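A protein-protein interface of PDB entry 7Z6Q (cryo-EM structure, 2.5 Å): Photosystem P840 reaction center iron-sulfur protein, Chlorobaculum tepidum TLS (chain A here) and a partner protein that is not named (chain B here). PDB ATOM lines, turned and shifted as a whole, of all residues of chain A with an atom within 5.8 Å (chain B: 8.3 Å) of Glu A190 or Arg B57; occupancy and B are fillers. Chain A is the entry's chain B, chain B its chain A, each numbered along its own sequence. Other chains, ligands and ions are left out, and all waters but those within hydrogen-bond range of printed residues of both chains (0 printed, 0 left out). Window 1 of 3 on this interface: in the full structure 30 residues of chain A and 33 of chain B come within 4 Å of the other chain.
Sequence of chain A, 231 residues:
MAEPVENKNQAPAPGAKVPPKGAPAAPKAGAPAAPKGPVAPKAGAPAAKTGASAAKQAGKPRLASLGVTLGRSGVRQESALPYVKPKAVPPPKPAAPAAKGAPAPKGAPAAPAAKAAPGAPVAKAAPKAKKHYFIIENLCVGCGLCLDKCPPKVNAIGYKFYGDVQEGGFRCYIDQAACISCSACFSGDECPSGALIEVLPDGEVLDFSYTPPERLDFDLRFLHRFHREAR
Arg B57 touches one residue of chain A.
Of the printed residues of chain B, Lys A149 touches Thr B56 (3.6 Å).
Of the printed residues of chain B, Asp A189 touches Asn B521.
Printed residues of chain B within 4 Å of Pro A192: Lys B519, Asn B521 and Leu B528.
Ser B524 touches none of the printed residues of chain A.
Cys A146 touches none of the printed residues of chain B.
The nearest residue of chain B that does not touch Glu A190 is Glu B55 (5.1 Å).
Among the printed residues, pairs that only touch across the chains: Phe A208 with Lys B519, Cys A143 with Leu B528, Glu A190 with Thr B56, Lys A149 with Thr B56, Pro A192 with Leu B528, Leu A145 with Thr B56, Pro A192 with Asn B521 and Glu A190 with Arg B57.
The backbone NH of Lys B519 sits at hydrogen-bond distance from the backbone carbonyl oxygen of Pro A192 (2.7 Å).
The backbone carbonyl oxygen of Asp A189 lies within hydrogen-bond range of the side-chain amide nitrogen of Asn B521, 2.6 Å away.
ND2 of Asn B521 lies within hydrogen-bond range of O of Glu A190.
ND2 of Asn B521 lies within hydrogen-bond range of O of Cys A191 (2.7 Å).
Of the 18 printed residues of chain B, 5 touch a printed residue of chain A.
Printed residues of chain B that touch a printed residue of chain A: Thr B56, Arg B57, Lys B519, Asn B521 and Leu B528.
Hydrophobic or aromatic side chains of chain B that line the printed part of chain A: Leu B528.
Hydrophobic or aromatic side chains of chain A that line the printed part of chain B: Leu A145, Pro A192 and Phe A208.
Among the printed residues, 12 pairs touch across the chains.
Among the printed residues, no Asp or Glu carboxylate lies within 4 Å of a Lys or Arg side-chain nitrogen of the other chain.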
ATOM      1  N   CYS A 143      13.732  -1.255  22.455  1.00  0.00           N
ATOM      2  CA  CYS A 143      13.013   0.012  22.379  1.00  0.00           C
ATOM      3  C   CYS A 143      13.609   1.074  23.293  1.00  0.00           C
ATOM      4  O   CYS A 143      13.344   2.264  23.094  1.00  0.00           O
ATOM      5  CB  CYS A 143      11.537  -0.199  22.712  1.00  0.00           C
ATOM      6  SG  CYS A 143      11.218  -0.832  24.369  1.00  0.00           S
ATOM      7  N   LEU A 145      13.008   2.024  26.284  1.00  0.00           N
ATOM      8  CA  LEU A 145      12.180   2.696  27.278  1.00  0.00           C
ATOM      9  C   LEU A 145      12.795   2.573  28.665  1.00  0.00           C
ATOM     10  O   LEU A 145      12.688   3.491  29.487  1.00  0.00           O
ATOM     11  CB  LEU A 145      10.768   2.115  27.258  1.00  0.00           C
ATOM     12  CG  LEU A 145       9.935   2.475  26.027  1.00  0.00           C
ATOM     13  CD1 LEU A 145       8.669   1.640  25.962  1.00  0.00           C
ATOM     14  CD2 LEU A 145       9.605   3.957  26.018  1.00  0.00           C
ATOM     15  N   CYS A 146      13.448   1.444  28.938  1.00  0.00           N
ATOM     16  CA  CYS A 146      14.138   1.258  30.208  1.00  0.00           C
ATOM     17  C   CYS A 146      15.326   2.203  30.345  1.00  0.00           C
ATOM     18  O   CYS A 146      15.588   2.727  31.432  1.00  0.00           O
ATOM     19  CB  CYS A 146      14.596  -0.194  30.334  1.00  0.00           C
ATOM     20  SG  CYS A 146      15.398  -0.849  28.854  1.00  0.00           S
ATOM     21  N   LYS A 149      14.690   5.694  31.845  1.00  0.00           N
ATOM     22  CA  LYS A 149      14.386   5.783  33.267  1.00  0.00           C
ATOM     23  C   LYS A 149      15.627   5.722  34.145  1.00  0.00           C
ATOM     24  O   LYS A 149      15.543   6.063  35.329  1.00  0.00           O
ATOM     25  CB  LYS A 149      13.420   4.674  33.682  1.00  0.00           C
ATOM     26  CG  LYS A 149      12.074   4.725  32.996  1.00  0.00           C
ATOM     27  CD  LYS A 149      11.310   5.944  33.481  1.00  0.00           C
ATOM     28  CE  LYS A 149       9.814   5.785  33.315  1.00  0.00           C
ATOM     29  NZ  LYS A 149       9.142   5.781  34.638  1.00  0.00           N
ATOM     30  N   CYS A 185      13.748   1.883  36.295  1.00  0.00           N
ATOM     31  CA  CYS A 185      13.385   1.189  35.031  1.00  0.00           C
ATOM     32  C   CYS A 185      12.226   0.214  35.264  1.00  0.00           C
ATOM     33  O   CYS A 185      11.358   0.114  34.380  1.00  0.00           O
ATOM     34  CB  CYS A 185      14.579   0.411  34.492  1.00  0.00           C
ATOM     35  SG  CYS A 185      15.375  -0.663  35.715  1.00  0.00           S
ATOM     36  N   PHE A 186      12.276  -0.553  36.359  1.00  0.00           N
ATOM     37  CA  PHE A 186      11.202  -1.529  36.679  1.00  0.00           C
ATOM     38  C   PHE A 186       9.895  -0.872  37.149  1.00  0.00           C
ATOM     39  O   PHE A 186       8.822  -1.308  36.680  1.00  0.00           O
ATOM     40  CB  PHE A 186      11.696  -2.600  37.654  1.00  0.00           C
ATOM     41  CG  PHE A 186      10.780  -3.793  37.725  1.00  0.00           C
ATOM     42  CD1 PHE A 186      10.652  -4.647  36.645  1.00  0.00           C
ATOM     43  CD2 PHE A 186      10.006  -4.026  38.846  1.00  0.00           C
ATOM     44  CE1 PHE A 186       9.789  -5.729  36.699  1.00  0.00           C
ATOM     45  CE2 PHE A 186       9.145  -5.110  38.897  1.00  0.00           C
ATOM     46  CZ  PHE A 186       9.040  -5.961  37.825  1.00  0.00           C
ATOM     47  N   GLY A 188       8.161   2.005  36.655  1.00  0.00           N
ATOM     48  CA  GLY A 188       7.320   2.380  35.538  1.00  0.00           C
ATOM     49  C   GLY A 188       7.163   1.168  34.647  1.00  0.00           C
ATOM     50  O   GLY A 188       8.166   0.588  34.196  1.00  0.00           O
ATOM     51  N   ASP A 189       5.924   0.770  34.374  1.00  0.00           N
ATOM     52  CA  ASP A 189       5.674  -0.457  33.629  1.00  0.00           C
ATOM     53  C   ASP A 189       5.931  -0.173  32.154  1.00  0.00           C
ATOM     54  O   ASP A 189       4.997  -0.134  31.347  1.00  0.00           O
ATOM     55  CB  ASP A 189       4.237  -0.920  33.851  1.00  0.00           C
ATOM     56  CG  ASP A 189       3.996  -1.398  35.267  1.00  0.00           C
ATOM     57  OD1 ASP A 189       4.953  -1.893  35.897  1.00  0.00           O
ATOM     58  OD2 ASP A 189       2.850  -1.284  35.750  1.00  0.00           O
ATOM     59  N   GLU A 190       7.202   0.020  31.800  1.00  0.00           N
ATOM     60  CA  GLU A 190       7.549   0.436  30.448  1.00  0.00           C
ATOM     61  C   GLU A 190       7.611  -0.786  29.543  1.00  0.00           C
ATOM     62  O   GLU A 190       7.115  -0.756  28.412  1.00  0.00           O
ATOM     63  CB  GLU A 190       8.888   1.172  30.424  1.00  0.00           C
ATOM     64  CG  GLU A 190       8.886   2.480  31.170  1.00  0.00           C
ATOM     65  CD  GLU A 190       7.845   3.440  30.640  1.00  0.00           C
ATOM     66  OE1 GLU A 190       7.672   3.505  29.404  1.00  0.00           O
ATOM     67  OE2 GLU A 190       7.202   4.130  31.457  1.00  0.00           O
ATOM     68  N   CYS A 191       8.213  -1.867  30.023  1.00  0.00           N
ATOM     69  CA  CYS A 191       8.641  -2.934  29.126  1.00  0.00           C
ATOM     70  C   CYS A 191       7.440  -3.633  28.500  1.00  0.00           C
ATOM     71  O   CYS A 191       6.536  -4.073  29.218  1.00  0.00           O
ATOM     72  CB  CYS A 191       9.514  -3.944  29.865  1.00  0.00           C
ATOM     73  SG  CYS A 191      10.192  -5.234  28.794  1.00  0.00           S
ATOM     74  N   PRO A 192       7.392  -3.745  27.174  1.00  0.00           N
ATOM     75  CA  PRO A 192       6.282  -4.423  26.496  1.00  0.00           C
ATOM     76  C   PRO A 192       6.481  -5.912  26.266  1.00  0.00           C
ATOM     77  O   PRO A 192       5.542  -6.575  25.812  1.00  0.00           O
ATOM     78  CB  PRO A 192       6.245  -3.685  25.155  1.00  0.00           C
ATOM     79  CG  PRO A 192       7.674  -3.407  24.896  1.00  0.00           C
ATOM     80  CD  PRO A 192       8.270  -3.048  26.220  1.00  0.00           C
ATOM     81  N   PHE A 208       6.706  -8.445  35.693  1.00  0.00           N
ATOM     82  CA  PHE A 208       5.876  -7.253  35.659  1.00  0.00           C
ATOM     83  C   PHE A 208       5.501  -6.878  37.086  1.00  0.00           C
ATOM     84  O   PHE A 208       5.438  -7.737  37.969  1.00  0.00           O
ATOM     85  CB  PHE A 208       4.621  -7.493  34.807  1.00  0.00           C
ATOM     86  CG  PHE A 208       3.942  -6.238  34.344  1.00  0.00           C
ATOM     87  CD1 PHE A 208       4.492  -5.469  33.333  1.00  0.00           C
ATOM     88  CD2 PHE A 208       2.744  -5.841  34.898  1.00  0.00           C
ATOM     89  CE1 PHE A 208       3.861  -4.320  32.896  1.00  0.00           C
ATOM     90  CE2 PHE A 208       2.109  -4.696  34.469  1.00  0.00           C
ATOM     91  CZ  PHE A 208       2.667  -3.935  33.467  1.00  0.00           C
ATOM     92  N   PHE B  51      16.438  13.224  28.709  1.00  0.00           N
ATOM     93  CA  PHE B  51      15.673  12.473  29.740  1.00  0.00           C
ATOM     94  C   PHE B  51      14.517  13.333  30.270  1.00  0.00           C
ATOM     95  O   PHE B  51      13.533  12.757  30.775  1.00  0.00           O
ATOM     96  CB  PHE B  51      16.594  11.990  30.864  1.00  0.00           C
ATOM     97  CG  PHE B  51      17.553  10.895  30.466  1.00  0.00           C
ATOM     98  CD1 PHE B  51      17.327  10.128  29.335  1.00  0.00           C
ATOM     99  CD2 PHE B  51      18.682  10.630  31.225  1.00  0.00           C
ATOM    100  CE1 PHE B  51      18.208   9.122  28.970  1.00  0.00           C
ATOM    101  CE2 PHE B  51      19.563   9.624  30.860  1.00  0.00           C
ATOM    102  CZ  PHE B  51      19.324   8.871  29.734  1.00  0.00           C
ATOM    103  N   THR B  54      11.191  12.815  27.395  1.00  0.00           N
ATOM    104  CA  THR B  54      11.226  11.385  26.972  1.00  0.00           C
ATOM    105  C   THR B  54       9.846  10.859  26.556  1.00  0.00           C
ATOM    106  O   THR B  54       8.851  11.563  26.749  1.00  0.00           O
ATOM    107  CB  THR B  54      11.828  10.482  28.056  1.00  0.00           C
ATOM    108  OG1 THR B  54      12.011   9.189  27.482  1.00  0.00           O
ATOM    109  CG2 THR B  54      10.969  10.390  29.300  1.00  0.00           C
ATOM    110  N   GLU B  55       9.822   9.635  26.016  1.00  0.00           N
ATOM    111  CA  GLU B  55       8.603   8.939  25.517  1.00  0.00           C
ATOM    112  C   GLU B  55       7.896   8.184  26.652  1.00  0.00           C
ATOM    113  O   GLU B  55       6.874   7.529  26.356  1.00  0.00           O
ATOM    114  CB  GLU B  55       8.974   7.899  24.453  1.00  0.00           C
ATOM    115  CG  GLU B  55       9.118   8.441  23.040  1.00  0.00           C
ATOM    116  CD  GLU B  55       7.824   8.775  22.315  1.00  0.00           C
ATOM    117  OE1 GLU B  55       7.369   7.954  21.489  1.00  0.00           O
ATOM    118  OE2 GLU B  55       7.282   9.863  22.570  1.00  0.00           O
ATOM    119  N   THR B  56       8.454   8.220  27.865  1.00  0.00           N
ATOM    120  CA  THR B  56       7.862   7.487  29.018  1.00  0.00           C
ATOM    121  C   THR B  56       6.763   8.334  29.668  1.00  0.00           C
ATOM    122  O   THR B  56       6.644   9.522  29.312  1.00  0.00           O
ATOM    123  CB  THR B  56       8.942   7.028  30.006  1.00  0.00           C
ATOM    124  OG1 THR B  56       9.704   8.161  30.423  1.00  0.00           O
ATOM    125  CG2 THR B  56       9.867   5.983  29.418  1.00  0.00           C
ATOM    126  N   ARG B  57       5.991   7.745  30.579  1.00  0.00           N
ATOM    127  CA  ARG B  57       4.906   8.449  31.262  1.00  0.00           C
ATOM    128  C   ARG B  57       5.421   9.651  32.048  1.00  0.00           C
ATOM    129  O   ARG B  57       6.426   9.552  32.755  1.00  0.00           O
ATOM    130  CB  ARG B  57       4.156   7.495  32.194  1.00  0.00           C
ATOM    131  CG  ARG B  57       2.980   8.128  32.919  1.00  0.00           C
ATOM    132  CD  ARG B  57       2.221   7.100  33.743  1.00  0.00           C
ATOM    133  NE  ARG B  57       2.780   6.953  35.084  1.00  0.00           N
ATOM    134  CZ  ARG B  57       2.120   6.434  36.114  1.00  0.00           C
ATOM    135  NH1 ARG B  57       2.707   6.339  37.299  1.00  0.00           N
ATOM    136  NH2 ARG B  57       0.873   6.012  35.961  1.00  0.00           N
ATOM    137  N   SER B  58       4.714  10.774  31.933  1.00  0.00           N
ATOM    138  CA  SER B  58       5.108  12.033  32.617  1.00  0.00           C
ATOM    139  C   SER B  58       3.912  12.989  32.646  1.00  0.00           C
ATOM    140  O   SER B  58       2.881  12.668  32.026  1.00  0.00           O
ATOM    141  CB  SER B  58       6.304  12.663  31.949  1.00  0.00           C
ATOM    142  OG  SER B  58       6.080  12.831  30.557  1.00  0.00           O
ATOM    143  N   THR B  59       4.051  14.114  33.353  1.00  0.00           N
ATOM    144  CA  THR B  59       2.959  15.119  33.445  1.00  0.00           C
ATOM    145  C   THR B  59       3.124  16.124  32.301  1.00  0.00           C
ATOM    146  O   THR B  59       4.240  16.642  32.142  1.00  0.00           O
ATOM    147  CB  THR B  59       3.015  15.885  34.772  1.00  0.00           C
ATOM    148  OG1 THR B  59       4.044  16.870  34.660  1.00  0.00           O
ATOM    149  CG2 THR B  59       3.278  14.996  35.967  1.00  0.00           C
ATOM    150  N   LYS B  60       2.050  16.401  31.557  1.00  0.00           N
ATOM    151  CA  LYS B  60       2.102  17.338  30.446  1.00  0.00           C
ATOM    152  C   LYS B  60       1.062  18.436  30.628  1.00  0.00           C
ATOM    153  O   LYS B  60       0.043  18.248  31.299  1.00  0.00           O
ATOM    154  CB  LYS B  60       1.877  16.589  29.135  1.00  0.00           C
ATOM    155  CG  LYS B  60       2.849  15.434  28.949  1.00  0.00           C
ATOM    156  CD  LYS B  60       2.454  14.540  27.793  1.00  0.00           C
ATOM    157  CE  LYS B  60       3.426  13.385  27.629  1.00  0.00           C
ATOM    158  NZ  LYS B  60       3.318  12.411  28.751  1.00  0.00           N
ATOM    159  N   GLN B  63      -2.748  17.811  30.086  1.00  0.00           N
ATOM    160  CA  GLN B  63      -3.400  16.726  30.811  1.00  0.00           C
ATOM    161  C   GLN B  63      -3.621  17.069  32.281  1.00  0.00           C
ATOM    162  O   GLN B  63      -3.663  16.163  33.115  1.00  0.00           O
ATOM    163  CB  GLN B  63      -2.584  15.433  30.730  1.00  0.00           C
ATOM    164  CG  GLN B  63      -2.380  14.852  29.354  1.00  0.00           C
ATOM    165  CD  GLN B  63      -1.351  13.743  29.369  1.00  0.00           C
ATOM    166  OE1 GLN B  63      -1.592  12.646  28.867  1.00  0.00           O
ATOM    167  NE2 GLN B  63      -0.201  14.015  29.973  1.00  0.00           N
ATOM    168  N   LEU B 400      -4.770  -3.289  32.240  1.00  0.00           N
ATOM    169  CA  LEU B 400      -3.529  -3.220  33.056  1.00  0.00           C
ATOM    170  C   LEU B 400      -3.810  -3.645  34.503  1.00  0.00           C
ATOM    171  O   LEU B 400      -2.957  -4.334  35.079  1.00  0.00           O
ATOM    172  CB  LEU B 400      -2.978  -1.793  33.003  1.00  0.00           C
ATOM    173  CG  LEU B 400      -2.338  -1.385  31.677  1.00  0.00           C
ATOM    174  CD1 LEU B 400      -1.734   0.008  31.773  1.00  0.00           C
ATOM    175  CD2 LEU B 400      -1.283  -2.392  31.251  1.00  0.00           C
ATOM    176  N   LYS B 519       3.066  -6.336  24.838  1.00  0.00           N
ATOM    177  CA  LYS B 519       1.993  -5.652  25.612  1.00  0.00           C
ATOM    178  C   LYS B 519       1.988  -4.175  25.220  1.00  0.00           C
ATOM    179  O   LYS B 519       3.076  -3.572  25.232  1.00  0.00           O
ATOM    180  CB  LYS B 519       2.278  -5.723  27.116  1.00  0.00           C
ATOM    181  CG  LYS B 519       1.306  -6.560  27.932  1.00  0.00           C
ATOM    182  CD  LYS B 519       1.515  -6.411  29.419  1.00  0.00           C
ATOM    183  CE  LYS B 519       2.824  -7.007  29.892  1.00  0.00           C
ATOM    184  NZ  LYS B 519       2.954  -6.955  31.369  1.00  0.00           N
ATOM    185  N   LYS B 520       0.804  -3.593  25.001  1.00  0.00           N
ATOM    186  CA  LYS B 520       0.677  -2.132  24.732  1.00  0.00           C
ATOM    187  C   LYS B 520       0.489  -1.457  26.098  1.00  0.00           C
ATOM    188  O   LYS B 520      -0.667  -1.148  26.449  1.00  0.00           O
ATOM    189  CB  LYS B 520      -0.524  -1.870  23.818  1.00  0.00           C
ATOM    190  CG  LYS B 520      -0.449  -2.522  22.443  1.00  0.00           C
ATOM    191  CD  LYS B 520      -1.651  -2.221  21.572  1.00  0.00           C
ATOM    192  CE  LYS B 520      -1.576  -2.881  20.211  1.00  0.00           C
ATOM    193  NZ  LYS B 520      -2.767  -2.570  19.386  1.00  0.00           N
ATOM    194  N   ASN B 521       1.589  -1.241  26.826  1.00  0.00           N
ATOM    195  CA  ASN B 521       1.521  -0.783  28.241  1.00  0.00           C
ATOM    196  C   ASN B 521       0.728   0.528  28.308  1.00  0.00           C
ATOM    197  O   ASN B 521       0.184   0.835  29.387  1.00  0.00           O
ATOM    198  CB  ASN B 521       2.913  -0.631  28.856  1.00  0.00           C
ATOM    199  CG  ASN B 521       3.608  -1.959  29.076  1.00  0.00           C
ATOM    200  OD1 ASN B 521       2.991  -3.015  28.964  1.00  0.00           O
ATOM    201  ND2 ASN B 521       4.894  -1.915  29.389  1.00  0.00           N
ATOM    202  N   SER B 522       0.670   1.264  27.192  1.00  0.00           N
ATOM    203  CA  SER B 522       0.464   2.736  27.228  1.00  0.00           C
ATOM    204  C   SER B 522      -0.450   3.164  26.074  1.00  0.00           C
ATOM    205  O   SER B 522      -0.564   2.399  25.095  1.00  0.00           O
ATOM    206  CB  SER B 522       1.780   3.468  27.188  1.00  0.00           C
ATOM    207  OG  SER B 522       1.605   4.838  27.516  1.00  0.00           O
ATOM    208  N   TYR B 523      -1.070   4.341  26.194  1.00  0.00           N
ATOM    209  CA  TYR B 523      -1.933   4.874  25.151  1.00  0.00           C
ATOM    210  C   TYR B 523      -1.223   5.854  24.228  1.00  0.00           C
ATOM    211  O   TYR B 523      -1.740   6.132  23.143  1.00  0.00           O
ATOM    212  CB  TYR B 523      -3.181   5.541  25.758  1.00  0.00           C
ATOM    213  CG  TYR B 523      -2.934   6.696  26.710  1.00  0.00           C
ATOM    214  CD1 TYR B 523      -2.532   7.940  26.243  1.00  0.00           C
ATOM    215  CD2 TYR B 523      -3.135   6.546  28.073  1.00  0.00           C
ATOM    216  CE1 TYR B 523      -2.315   8.992  27.107  1.00  0.00           C
ATOM    217  CE2 TYR B 523      -2.922   7.594  28.945  1.00  0.00           C
ATOM    218  CZ  TYR B 523      -2.512   8.814  28.456  1.00  0.00           C
ATOM    219  OH  TYR B 523      -2.299   9.860  29.322  1.00  0.00           O
ATOM    220  N   SER B 524      -0.054   6.359  24.611  1.00  0.00           N
ATOM    221  CA  SER B 524       0.665   7.362  23.833  1.00  0.00           C
ATOM    222  C   SER B 524       2.126   6.962  23.650  1.00  0.00           C
ATOM    223  O   SER B 524       3.044   7.759  23.851  1.00  0.00           O
ATOM    224  CB  SER B 524       0.561   8.732  24.493  1.00  0.00           C
ATOM    225  OG  SER B 524       1.435   8.832  25.602  1.00  0.00           O
ATOM    226  N   PHE B 525       2.364   5.701  23.261  1.00  0.00           N
ATOM    227  CA  PHE B 525       3.731   5.295  22.969  1.00  0.00           C
ATOM    228  C   PHE B 525       3.942   5.185  21.463  1.00  0.00           C
ATOM    229  O   PHE B 525       3.137   4.559  20.763  1.00  0.00           O
ATOM    230  CB  PHE B 525       4.083   3.962  23.642  1.00  0.00           C
ATOM    231  CG  PHE B 525       3.343   2.787  23.091  1.00  0.00           C
ATOM    232  CD1 PHE B 525       2.033   2.545  23.453  1.00  0.00           C
ATOM    233  CD2 PHE B 525       3.967   1.910  22.226  1.00  0.00           C
ATOM    234  CE1 PHE B 525       1.356   1.460  22.951  1.00  0.00           C
ATOM    235  CE2 PHE B 525       3.297   0.826  21.726  1.00  0.00           C
ATOM    236  CZ  PHE B 525       1.987   0.600  22.087  1.00  0.00           C
ATOM    237  N   LEU B 528       7.677   0.629  18.944  1.00  0.00           N
ATOM    238  CA  LEU B 528       8.545  -0.213  19.806  1.00  0.00           C
ATOM    239  C   LEU B 528       9.978  -0.161  19.260  1.00  0.00           C
ATOM    240  O   LEU B 528      10.862  -0.786  19.868  1.00  0.00           O
ATOM    241  CB  LEU B 528       7.994  -1.640  19.843  1.00  0.00           C
ATOM    242  CG  LEU B 528       6.749  -1.812  20.710  1.00  0.00           C
ATOM    243  CD1 LEU B 528       6.429  -3.283  20.912  1.00  0.00           C
ATOM    244  CD2 LEU B 528       6.927  -1.111  22.046  1.00  0.00           C
